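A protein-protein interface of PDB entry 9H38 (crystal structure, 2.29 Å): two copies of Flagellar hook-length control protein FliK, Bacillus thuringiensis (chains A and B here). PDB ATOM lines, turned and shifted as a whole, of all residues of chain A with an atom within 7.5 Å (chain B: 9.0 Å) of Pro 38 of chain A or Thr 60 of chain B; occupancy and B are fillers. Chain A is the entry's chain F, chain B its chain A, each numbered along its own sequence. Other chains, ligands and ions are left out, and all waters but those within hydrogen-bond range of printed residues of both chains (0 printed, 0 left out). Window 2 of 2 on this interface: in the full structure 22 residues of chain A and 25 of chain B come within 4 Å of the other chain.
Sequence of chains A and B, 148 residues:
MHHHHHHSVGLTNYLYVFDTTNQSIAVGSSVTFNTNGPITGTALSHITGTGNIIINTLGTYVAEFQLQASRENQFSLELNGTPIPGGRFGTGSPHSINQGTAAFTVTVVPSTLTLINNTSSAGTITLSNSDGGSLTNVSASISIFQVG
The backbone carbonyl oxygen of Thr 60 of chain B is in hydrogen-bond range of the backbone NH of Gly 148 of chain B (3.0 Å).
The backbone carbonyl oxygen of Phe 104 of chain B sits at hydrogen-bond distance from the backbone NH of Tyr 61 of chain B.
N of Ala 63 of chain B is in hydrogen-bond range of O of Ala 102 of chain B (2.7 Å).
N of Thr 40 of chain A sits at hydrogen-bond distance from O of Tyr 14 of chain A (2.8 Å).
The backbone carbonyl oxygen (O) of Tyr 16 of chain A lies within hydrogen-bond range of the backbone NH (N) of Gly 37 of chain A.
N of Tyr 16 of chain A lies within hydrogen-bond range of O of Pro 38 of chain A (3.2 Å).
1 position is printed for both chains.
Of the 10 pairs that touch across the chains among the printed residues, none has its exchanged pair printed and touching as well.
Of the 11 printed residues of chain A, 4 touch a printed residue of chain B.
Printed residues of chain A that touch a printed residue of chain B: Tyr 14, Tyr 16, Phe 18 and Pro 38.
Hydrophobic or aromatic side chains of chain A that line the printed part of chain B: Tyr 14, Tyr 16, Phe 18 and Pro 38.
Of the 24 printed residues of chain B, 7 touch a printed residue of chain A.
Printed residues of chain B that touch a printed residue of chain A: Thr 60, Val 62, Pro 85, Gly 86, Ala 102, Ala 103 and Phe 104.
Hydrophobic or aromatic side chains of chain B within 4 Å of the printed part of chain A: Val 62, Ala 102 and Ala 103.
Among the printed residues, no Asp or Glu carboxylate lies within 4 Å of a Lys or Arg side-chain nitrogen of the other chain.
Among the printed residues, merely in contact across the chains: Pro 38 of chain A with Ala 103 of chain B (3.0 Å), Tyr 14 of chain A with Ala 103 of chain B (3.2 Å), Phe 18 of chain A with Gly 86 of chain B (3.4 Å), Tyr 14 of chain A with Val 62 of chain B (3.4 Å), Tyr 16 of chain A with Ala 103 of chain B (3.6 Å), Pro 38 of chain A with Thr 60 of chain B (3.6 Å), Tyr 16 of chain A with Ala 102 of chain B (3.7 Å), Pro 38 of chain A with Phe 104 of chain B (3.8 Å) and Phe 18 of chain A with Pro 85 of chain B (3.8 Å).
O of Gly 86 of chain B is in hydrogen-bond range of OH of Tyr 16 of chain A, 2.8 Å away.
Of chain B, only Thr 60, Ala 103 and Phe 104 come within 4 Å of Pro 38 of chain A.
Of chain A, only Pro 38 (3.6 Å) comes within 4 Å of Thr 60 of chain B.
No residue of chain B comes within 4 Å of Gly 37 of chain A.
No residue of chain B comes within 4 Å of Ile 39 of chain A.
Of the printed residues of chain B, Phe 18 of chain A touches Pro 85 and Gly 86.
Of the printed residues of chain A, Val 62 of chain B touches Tyr 14 (3.4 Å).
Of the printed residues of chain A, Phe 104 of chain B touches Pro 38.
Printed residues of chain B within 4 Å of Tyr 16 of chain A: Gly 86 (2.8 Å), Ala 102 (3.7 Å) and Ala 103 (3.6 Å).
Ile 84 of chain B touches none of the printed residues of chain A.
Leu 58 of chain B touches none of the printed residues of chain A.
The nearest printed residue of chain A that does not touch Gly 86 of chain B is Gly 37 of chain A (7.2 Å).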
ATOM      1  N   TYR A  14     -19.326  -5.417   9.181  1.00  0.00           N
ATOM      2  CA  TYR A  14     -18.812  -6.373   8.209  1.00  0.00           C
ATOM      3  C   TYR A  14     -19.129  -5.907   6.800  1.00  0.00           C
ATOM      4  O   TYR A  14     -20.225  -5.407   6.537  1.00  0.00           O
ATOM      5  CB  TYR A  14     -19.408  -7.770   8.398  1.00  0.00           C
ATOM      6  CG  TYR A  14     -18.971  -8.681   7.291  1.00  0.00           C
ATOM      7  CD1 TYR A  14     -17.755  -9.331   7.364  1.00  0.00           C
ATOM      8  CD2 TYR A  14     -19.749  -8.862   6.159  1.00  0.00           C
ATOM      9  CE1 TYR A  14     -17.320 -10.142   6.354  1.00  0.00           C
ATOM     10  CE2 TYR A  14     -19.316  -9.677   5.131  1.00  0.00           C
ATOM     11  CZ  TYR A  14     -18.093 -10.317   5.234  1.00  0.00           C
ATOM     12  OH  TYR A  14     -17.639 -11.147   4.218  1.00  0.00           O
ATOM     13  N   LEU A  15     -18.189  -6.135   5.883  1.00  0.00           N
ATOM     14  CA  LEU A  15     -18.402  -5.780   4.490  1.00  0.00           C
ATOM     15  C   LEU A  15     -17.720  -6.802   3.588  1.00  0.00           C
ATOM     16  O   LEU A  15     -16.577  -7.201   3.842  1.00  0.00           O
ATOM     17  CB  LEU A  15     -17.872  -4.372   4.198  1.00  0.00           C
ATOM     18  CG  LEU A  15     -17.680  -3.948   2.733  1.00  0.00           C
ATOM     19  CD1 LEU A  15     -18.036  -2.487   2.566  1.00  0.00           C
ATOM     20  CD2 LEU A  15     -16.237  -4.191   2.270  1.00  0.00           C
ATOM     21  N   TYR A  16     -18.425  -7.202   2.523  1.00  0.00           N
ATOM     22  CA  TYR A  16     -17.872  -8.025   1.458  1.00  0.00           C
ATOM     23  C   TYR A  16     -18.073  -7.303   0.133  1.00  0.00           C
ATOM     24  O   TYR A  16     -19.194  -6.885  -0.175  1.00  0.00           O
ATOM     25  CB  TYR A  16     -18.545  -9.400   1.424  1.00  0.00           C
ATOM     26  CG  TYR A  16     -18.061 -10.324   0.323  1.00  0.00           C
ATOM     27  CD1 TYR A  16     -16.711 -10.526   0.109  1.00  0.00           C
ATOM     28  CD2 TYR A  16     -18.956 -10.985  -0.505  1.00  0.00           C
ATOM     29  CE1 TYR A  16     -16.256 -11.364  -0.884  1.00  0.00           C
ATOM     30  CE2 TYR A  16     -18.508 -11.819  -1.512  1.00  0.00           C
ATOM     31  CZ  TYR A  16     -17.149 -12.001  -1.693  1.00  0.00           C
ATOM     32  OH  TYR A  16     -16.667 -12.834  -2.686  1.00  0.00           O
ATOM     33  N   VAL A  17     -16.988  -7.141  -0.642  1.00  0.00           N
ATOM     34  CA  VAL A  17     -17.050  -6.614  -2.002  1.00  0.00           C
ATOM     35  C   VAL A  17     -16.264  -7.541  -2.925  1.00  0.00           C
ATOM     36  O   VAL A  17     -15.285  -8.172  -2.512  1.00  0.00           O
ATOM     37  CB  VAL A  17     -16.522  -5.164  -2.110  1.00  0.00           C
ATOM     38  CG1 VAL A  17     -17.351  -4.211  -1.226  1.00  0.00           C
ATOM     39  CG2 VAL A  17     -15.056  -5.087  -1.760  1.00  0.00           C
ATOM     40  N   PHE A  18     -16.716  -7.646  -4.179  1.00  0.00           N
ATOM     41  CA  PHE A  18     -16.024  -8.489  -5.146  1.00  0.00           C
ATOM     42  C   PHE A  18     -16.183  -7.932  -6.553  1.00  0.00           C
ATOM     43  O   PHE A  18     -17.058  -7.103  -6.827  1.00  0.00           O
ATOM     44  CB  PHE A  18     -16.512  -9.942  -5.104  1.00  0.00           C
ATOM     45  CG  PHE A  18     -17.969 -10.119  -5.428  1.00  0.00           C
ATOM     46  CD1 PHE A  18     -18.932  -9.991  -4.442  1.00  0.00           C
ATOM     47  CD2 PHE A  18     -18.372 -10.470  -6.710  1.00  0.00           C
ATOM     48  CE1 PHE A  18     -20.289 -10.175  -4.735  1.00  0.00           C
ATOM     49  CE2 PHE A  18     -19.728 -10.653  -7.013  1.00  0.00           C
ATOM     50  CZ  PHE A  18     -20.687 -10.514  -6.012  1.00  0.00           C
ATOM     51  N   ASN A  36     -21.358  -5.429  -4.575  1.00  0.00           N
ATOM     52  CA  ASN A  36     -21.372  -5.430  -3.119  1.00  0.00           C
ATOM     53  C   ASN A  36     -22.003  -6.716  -2.614  1.00  0.00           C
ATOM     54  O   ASN A  36     -23.108  -7.082  -3.035  1.00  0.00           O
ATOM     55  CB  ASN A  36     -22.150  -4.239  -2.572  1.00  0.00           C
ATOM     56  CG  ASN A  36     -21.330  -2.992  -2.557  1.00  0.00           C
ATOM     57  OD1 ASN A  36     -20.202  -2.983  -3.065  1.00  0.00           O
ATOM     58  ND2 ASN A  36     -21.889  -1.913  -2.000  1.00  0.00           N
ATOM     59  N   GLY A  37     -21.304  -7.395  -1.720  1.00  0.00           N
ATOM     60  CA  GLY A  37     -21.910  -8.475  -0.995  1.00  0.00           C
ATOM     61  C   GLY A  37     -22.702  -7.935   0.178  1.00  0.00           C
ATOM     62  O   GLY A  37     -23.019  -6.743   0.267  1.00  0.00           O
ATOM     63  N   PRO A  38     -23.037  -8.825   1.105  1.00  0.00           N
ATOM     64  CA  PRO A  38     -23.660  -8.383   2.353  1.00  0.00           C
ATOM     65  C   PRO A  38     -22.783  -7.381   3.088  1.00  0.00           C
ATOM     66  O   PRO A  38     -21.561  -7.530   3.154  1.00  0.00           O
ATOM     67  CB  PRO A  38     -23.813  -9.687   3.141  1.00  0.00           C
ATOM     68  CG  PRO A  38     -23.996 -10.719   2.054  1.00  0.00           C
ATOM     69  CD  PRO A  38     -23.072 -10.286   0.946  1.00  0.00           C
ATOM     70  N   ILE A  39     -23.428  -6.341   3.613  1.00  0.00           N
ATOM     71  CA  ILE A  39     -22.812  -5.344   4.475  1.00  0.00           C
ATOM     72  C   ILE A  39     -23.666  -5.209   5.720  1.00  0.00           C
ATOM     73  O   ILE A  39     -24.869  -4.954   5.621  1.00  0.00           O
ATOM     74  CB  ILE A  39     -22.689  -3.969   3.793  1.00  0.00           C
ATOM     75  CG1 ILE A  39     -21.810  -4.037   2.549  1.00  0.00           C
ATOM     76  CG2 ILE A  39     -22.144  -2.925   4.785  1.00  0.00           C
ATOM     77  CD1 ILE A  39     -21.799  -2.739   1.815  1.00  0.00           C
ATOM     78  N   THR A  40     -23.047  -5.356   6.882  1.00  0.00           N
ATOM     79  CA  THR A  40     -23.695  -5.103   8.155  1.00  0.00           C
ATOM     80  C   THR A  40     -23.047  -3.896   8.826  1.00  0.00           C
ATOM     81  O   THR A  40     -21.901  -3.534   8.531  1.00  0.00           O
ATOM     82  CB  THR A  40     -23.612  -6.333   9.074  1.00  0.00           C
ATOM     83  OG1 THR A  40     -22.260  -6.525   9.509  1.00  0.00           O
ATOM     84  CG2 THR A  40     -24.102  -7.597   8.347  1.00  0.00           C
ATOM     85  N   ILE A 144     -13.920  -7.893   5.022  1.00  0.00           N
ATOM     86  CA  ILE A 144     -13.334  -7.110   6.112  1.00  0.00           C
ATOM     87  C   ILE A 144     -14.354  -6.928   7.223  1.00  0.00           C
ATOM     88  O   ILE A 144     -15.539  -6.731   6.958  1.00  0.00           O
ATOM     89  CB  ILE A 144     -12.822  -5.732   5.624  1.00  0.00           C
ATOM     90  CG1 ILE A 144     -12.330  -4.871   6.791  1.00  0.00           C
ATOM     91  CG2 ILE A 144     -13.898  -4.983   4.899  1.00  0.00           C
ATOM     92  CD1 ILE A 144     -11.653  -3.558   6.356  1.00  0.00           C
ATOM     93  N   ASN B  13     -22.229 -17.962  16.371  1.00  0.00           N
ATOM     94  CA  ASN B  13     -22.405 -19.200  15.633  1.00  0.00           C
ATOM     95  C   ASN B  13     -21.177 -19.414  14.759  1.00  0.00           C
ATOM     96  O   ASN B  13     -20.849 -18.559  13.931  1.00  0.00           O
ATOM     97  CB  ASN B  13     -23.679 -19.154  14.793  1.00  0.00           C
ATOM     98  CG  ASN B  13     -24.923 -19.355  15.625  1.00  0.00           C
ATOM     99  OD1 ASN B  13     -25.107 -20.406  16.233  1.00  0.00           O
ATOM    100  ND2 ASN B  13     -25.779 -18.334  15.675  1.00  0.00           N
ATOM    101  N   LEU B  44     -25.541 -23.808  13.158  1.00  0.00           N
ATOM    102  CA  LEU B  44     -24.816 -24.527  12.124  1.00  0.00           C
ATOM    103  C   LEU B  44     -24.589 -25.975  12.527  1.00  0.00           C
ATOM    104  O   LEU B  44     -24.251 -26.259  13.678  1.00  0.00           O
ATOM    105  CB  LEU B  44     -23.478 -23.849  11.834  1.00  0.00           C
ATOM    106  CG  LEU B  44     -23.621 -22.411  11.343  1.00  0.00           C
ATOM    107  CD1 LEU B  44     -22.327 -21.610  11.553  1.00  0.00           C
ATOM    108  CD2 LEU B  44     -24.053 -22.393   9.881  1.00  0.00           C
ATOM    109  N   ILE B  55     -28.051 -24.609   7.984  1.00  0.00           N
ATOM    110  CA  ILE B  55     -28.106 -23.292   8.607  1.00  0.00           C
ATOM    111  C   ILE B  55     -29.526 -23.068   9.099  1.00  0.00           C
ATOM    112  O   ILE B  55     -30.450 -22.920   8.285  1.00  0.00           O
ATOM    113  CB  ILE B  55     -27.711 -22.179   7.630  1.00  0.00           C
ATOM    114  CG1 ILE B  55     -26.327 -22.438   7.037  1.00  0.00           C
ATOM    115  CG2 ILE B  55     -27.852 -20.798   8.308  1.00  0.00           C
ATOM    116  CD1 ILE B  55     -25.908 -21.352   6.090  1.00  0.00           C
ATOM    117  N   THR B  57     -30.545 -20.589  11.453  1.00  0.00           N
ATOM    118  CA  THR B  57     -30.822 -19.255  11.955  1.00  0.00           C
ATOM    119  C   THR B  57     -30.717 -18.266  10.807  1.00  0.00           C
ATOM    120  O   THR B  57     -29.759 -18.305  10.025  1.00  0.00           O
ATOM    121  CB  THR B  57     -29.865 -18.888  13.094  1.00  0.00           C
ATOM    122  OG1 THR B  57     -30.219 -19.653  14.253  1.00  0.00           O
ATOM    123  CG2 THR B  57     -29.937 -17.398  13.418  1.00  0.00           C
ATOM    124  N   LEU B  58     -31.718 -17.399  10.689  1.00  0.00           N
ATOM    125  CA  LEU B  58     -31.708 -16.411   9.625  1.00  0.00           C
ATOM    126  C   LEU B  58     -30.582 -15.415   9.871  1.00  0.00           C
ATOM    127  O   LEU B  58     -30.242 -15.111  11.018  1.00  0.00           O
ATOM    128  CB  LEU B  58     -33.057 -15.690   9.558  1.00  0.00           C
ATOM    129  CG  LEU B  58     -34.251 -16.457   8.983  1.00  0.00           C
ATOM    130  CD1 LEU B  58     -35.459 -15.572   8.958  1.00  0.00           C
ATOM    131  CD2 LEU B  58     -33.946 -16.919   7.605  1.00  0.00           C
ATOM    132  N   GLY B  59     -29.991 -14.920   8.797  1.00  0.00           N
ATOM    133  CA  GLY B  59     -29.013 -13.865   8.940  1.00  0.00           C
ATOM    134  C   GLY B  59     -27.929 -13.951   7.890  1.00  0.00           C
ATOM    135  O   GLY B  59     -28.105 -14.567   6.843  1.00  0.00           O
ATOM    136  N   THR B  60     -26.802 -13.316   8.217  1.00  0.00           N
ATOM    137  CA  THR B  60     -25.706 -13.092   7.282  1.00  0.00           C
ATOM    138  C   THR B  60     -24.448 -13.805   7.764  1.00  0.00           C
ATOM    139  O   THR B  60     -23.988 -13.564   8.884  1.00  0.00           O
ATOM    140  CB  THR B  60     -25.461 -11.596   7.127  1.00  0.00           C
ATOM    141  OG1 THR B  60     -26.608 -11.013   6.503  1.00  0.00           O
ATOM    142  CG2 THR B  60     -24.221 -11.315   6.292  1.00  0.00           C
ATOM    143  N   TYR B  61     -23.885 -14.664   6.911  1.00  0.00           N
ATOM    144  CA  TYR B  61     -22.758 -15.520   7.259  1.00  0.00           C
ATOM    145  C   TYR B  61     -21.560 -15.271   6.338  1.00  0.00           C
ATOM    146  O   TYR B  61     -21.721 -14.950   5.157  1.00  0.00           O
ATOM    147  CB  TYR B  61     -23.171 -16.998   7.194  1.00  0.00           C
ATOM    148  CG  TYR B  61     -24.272 -17.386   8.166  1.00  0.00           C
ATOM    149  CD1 TYR B  61     -25.609 -17.157   7.862  1.00  0.00           C
ATOM    150  CD2 TYR B  61     -23.975 -17.985   9.380  1.00  0.00           C
ATOM    151  CE1 TYR B  61     -26.618 -17.503   8.740  1.00  0.00           C
ATOM    152  CE2 TYR B  61     -24.975 -18.347  10.259  1.00  0.00           C
ATOM    153  CZ  TYR B  61     -26.299 -18.100   9.940  1.00  0.00           C
ATOM    154  OH  TYR B  61     -27.307 -18.450  10.821  1.00  0.00           O
ATOM    155  N   VAL B  62     -20.350 -15.405   6.886  1.00  0.00           N
ATOM    156  CA  VAL B  62     -19.116 -15.368   6.102  1.00  0.00           C
ATOM    157  C   VAL B  62     -18.565 -16.789   5.973  1.00  0.00           C
ATOM    158  O   VAL B  62     -18.259 -17.438   6.982  1.00  0.00           O
ATOM    159  CB  VAL B  62     -18.065 -14.445   6.742  1.00  0.00           C
ATOM    160  CG1 VAL B  62     -16.883 -14.228   5.778  1.00  0.00           C
ATOM    161  CG2 VAL B  62     -18.706 -13.136   7.153  1.00  0.00           C
ATOM    162  N   ALA B  63     -18.376 -17.255   4.742  1.00  0.00           N
ATOM    163  CA  ALA B  63     -17.871 -18.602   4.499  1.00  0.00           C
ATOM    164  C   ALA B  63     -16.542 -18.551   3.750  1.00  0.00           C
ATOM    165  O   ALA B  63     -16.453 -17.997   2.641  1.00  0.00           O
ATOM    166  CB  ALA B  63     -18.887 -19.433   3.718  1.00  0.00           C
ATOM    167  N   ILE B  84     -24.107 -18.969  -5.070  1.00  0.00           N
ATOM    168  CA  ILE B  84     -24.158 -17.732  -4.282  1.00  0.00           C
ATOM    169  C   ILE B  84     -23.484 -16.609  -5.066  1.00  0.00           C
ATOM    170  O   ILE B  84     -22.429 -16.841  -5.689  1.00  0.00           O
ATOM    171  CB  ILE B  84     -23.465 -17.968  -2.934  1.00  0.00           C
ATOM    172  CG1 ILE B  84     -24.421 -18.615  -1.932  1.00  0.00           C
ATOM    173  CG2 ILE B  84     -22.807 -16.721  -2.394  1.00  0.00           C
ATOM    174  CD1 ILE B  84     -23.688 -19.260  -0.746  1.00  0.00           C
ATOM    175  N   PRO B  85     -24.030 -15.393  -5.080  1.00  0.00           N
ATOM    176  CA  PRO B  85     -23.351 -14.311  -5.801  1.00  0.00           C
ATOM    177  C   PRO B  85     -22.020 -14.016  -5.136  1.00  0.00           C
ATOM    178  O   PRO B  85     -21.927 -13.925  -3.912  1.00  0.00           O
ATOM    179  CB  PRO B  85     -24.323 -13.127  -5.698  1.00  0.00           C
ATOM    180  CG  PRO B  85     -25.608 -13.699  -5.180  1.00  0.00           C
ATOM    181  CD  PRO B  85     -25.275 -14.953  -4.441  1.00  0.00           C
ATOM    182  N   GLY B  86     -20.981 -13.894  -5.948  1.00  0.00           N
ATOM    183  CA  GLY B  86     -19.670 -13.722  -5.361  1.00  0.00           C
ATOM    184  C   GLY B  86     -19.123 -14.955  -4.684  1.00  0.00           C
ATOM    185  O   GLY B  86     -18.251 -14.845  -3.824  1.00  0.00           O
ATOM    186  N   ALA B 102     -16.434 -15.613   0.850  1.00  0.00           N
ATOM    187  CA  ALA B 102     -17.659 -14.940   0.428  1.00  0.00           C
ATOM    188  C   ALA B 102     -18.630 -14.848   1.596  1.00  0.00           C
ATOM    189  O   ALA B 102     -18.600 -15.679   2.503  1.00  0.00           O
ATOM    190  CB  ALA B 102     -18.359 -15.667  -0.725  1.00  0.00           C
ATOM    191  N   ALA B 103     -19.510 -13.840   1.551  1.00  0.00           N
ATOM    192  CA  ALA B 103     -20.570 -13.667   2.539  1.00  0.00           C
ATOM    193  C   ALA B 103     -21.942 -13.686   1.869  1.00  0.00           C
ATOM    194  O   ALA B 103     -22.116 -13.174   0.758  1.00  0.00           O
ATOM    195  CB  ALA B 103     -20.412 -12.367   3.312  1.00  0.00           C
ATOM    196  N   PHE B 104     -22.911 -14.285   2.549  1.00  0.00           N
ATOM    197  CA  PHE B 104     -24.235 -14.462   1.987  1.00  0.00           C
ATOM    198  C   PHE B 104     -25.262 -14.259   3.089  1.00  0.00           C
ATOM    199  O   PHE B 104     -24.954 -14.289   4.288  1.00  0.00           O
ATOM    200  CB  PHE B 104     -24.395 -15.848   1.326  1.00  0.00           C
ATOM    201  CG  PHE B 104     -24.121 -17.010   2.252  1.00  0.00           C
ATOM    202  CD1 PHE B 104     -22.815 -17.462   2.467  1.00  0.00           C
ATOM    203  CD2 PHE B 104     -25.156 -17.669   2.896  1.00  0.00           C
ATOM    204  CE1 PHE B 104     -22.565 -18.538   3.317  1.00  0.00           C
ATOM    205  CE2 PHE B 104     -24.902 -18.745   3.746  1.00  0.00           C
ATOM    206  CZ  PHE B 104     -23.615 -19.167   3.963  1.00  0.00           C
ATOM    207  N   THR B 105     -26.489 -14.055   2.676  1.00  0.00           N
ATOM    208  CA  THR B 105     -27.571 -13.854   3.616  1.00  0.00           C
ATOM    209  C   THR B 105     -28.531 -15.024   3.491  1.00  0.00           C
ATOM    210  O   THR B 105     -28.935 -15.373   2.378  1.00  0.00           O
ATOM    211  CB  THR B 105     -28.265 -12.511   3.360  1.00  0.00           C
ATOM    212  OG1 THR B 105     -27.535 -11.471   4.036  1.00  0.00           O
ATOM    213  CG2 THR B 105     -29.669 -12.532   3.896  1.00  0.00           C
ATOM    214  N   VAL B 106     -28.847 -15.660   4.621  1.00  0.00           N
ATOM    215  CA  VAL B 106     -29.819 -16.751   4.665  1.00  0.00           C
ATOM    216  C   VAL B 106     -31.191 -16.143   4.925  1.00  0.00           C
ATOM    217  O   VAL B 106     -31.423 -15.532   5.977  1.00  0.00           O
ATOM    218  CB  VAL B 106     -29.465 -17.785   5.743  1.00  0.00           C
ATOM    219  CG1 VAL B 106     -30.568 -18.794   5.877  1.00  0.00           C
ATOM    220  CG2 VAL B 106     -28.161 -18.482   5.410  1.00  0.00           C
ATOM    221  N   THR B 107     -32.100 -16.309   3.968  1.00  0.00           N
ATOM    222  CA  THR B 107     -33.422 -15.704   4.043  1.00  0.00           C
ATOM    223  C   THR B 107     -34.517 -16.696   4.410  1.00  0.00           C
ATOM    224  O   THR B 107     -35.635 -16.269   4.724  1.00  0.00           O
ATOM    225  CB  THR B 107     -33.777 -15.051   2.712  1.00  0.00           C
ATOM    226  OG1 THR B 107     -33.673 -16.031   1.677  1.00  0.00           O
ATOM    227  CG2 THR B 107     -32.803 -13.942   2.418  1.00  0.00           C
ATOM    228  N   ILE B 144     -16.969 -21.110   8.704  1.00  0.00           N
ATOM    229  CA  ILE B 144     -18.066 -20.157   8.524  1.00  0.00           C
ATOM    230  C   ILE B 144     -18.534 -19.627   9.875  1.00  0.00           C
ATOM    231  O   ILE B 144     -18.562 -20.356  10.874  1.00  0.00           O
ATOM    232  CB  ILE B 144     -19.248 -20.774   7.729  1.00  0.00           C
ATOM    233  CG1 ILE B 144     -20.509 -19.910   7.825  1.00  0.00           C
ATOM    234  CG2 ILE B 144     -19.555 -22.166   8.198  1.00  0.00           C
ATOM    235  CD1 ILE B 144     -21.663 -20.411   6.945  1.00  0.00           C
ATOM    236  N   PHE B 145     -18.896 -18.346   9.902  1.00  0.00           N
ATOM    237  CA  PHE B 145     -19.452 -17.720  11.094  1.00  0.00           C
ATOM    238  C   PHE B 145     -20.519 -16.714  10.691  1.00  0.00           C
ATOM    239  O   PHE B 145     -20.584 -16.269   9.545  1.00  0.00           O
ATOM    240  CB  PHE B 145     -18.371 -17.041  11.980  1.00  0.00           C
ATOM    241  CG  PHE B 145     -17.519 -16.003  11.277  1.00  0.00           C
ATOM    242  CD1 PHE B 145     -17.959 -14.698  11.130  1.00  0.00           C
ATOM    243  CD2 PHE B 145     -16.238 -16.316  10.852  1.00  0.00           C
ATOM    244  CE1 PHE B 145     -17.153 -13.729  10.519  1.00  0.00           C
ATOM    245  CE2 PHE B 145     -15.421 -15.363  10.242  1.00  0.00           C
ATOM    246  CZ  PHE B 145     -15.878 -14.067  10.071  1.00  0.00           C
ATOM    247  N   GLN B 146     -21.342 -16.344  11.671  1.00  0.00           N
ATOM    248  CA  GLN B 146     -22.502 -15.480  11.488  1.00  0.00           C
ATOM    249  C   GLN B 146     -22.157 -14.056  11.882  1.00  0.00           C
ATOM    250  O   GLN B 146     -21.799 -13.804  13.034  1.00  0.00           O
ATOM    251  CB  GLN B 146     -23.664 -15.972  12.347  1.00  0.00           C
ATOM    252  CG  GLN B 146     -24.963 -15.308  12.033  1.00  0.00           C
ATOM    253  CD  GLN B 146     -25.987 -15.527  13.118  1.00  0.00           C
ATOM    254  OE1 GLN B 146     -25.694 -16.142  14.153  1.00  0.00           O
ATOM    255  NE2 GLN B 146     -27.202 -15.039  12.891  1.00  0.00           N
ATOM    256  N   VAL B 147     -22.286 -13.124  10.944  1.00  0.00           N
ATOM    257  CA  VAL B 147     -22.058 -11.722  11.267  1.00  0.00           C
ATOM    258  C   VAL B 147     -23.351 -10.946  11.490  1.00  0.00           C
ATOM    259  O   VAL B 147     -23.322  -9.904  12.165  1.00  0.00           O
ATOM    260  CB  VAL B 147     -21.212 -11.029  10.183  1.00  0.00           C
ATOM    261  CG1 VAL B 147     -19.874 -11.678  10.101  1.00  0.00           C
ATOM    262  CG2 VAL B 147     -21.898 -11.072   8.847  1.00  0.00           C
ATOM    263  N   GLY B 148     -24.476 -11.404  10.944  1.00  0.00           N
ATOM    264  CA  GLY B 148     -25.733 -10.683  11.101  1.00  0.00           C
ATOM    265  C   GLY B 148     -26.968 -11.538  11.345  1.00  0.00           C
ATOM    266  O   GLY B 148     -26.945 -12.774  11.233  1.00  0.00           O
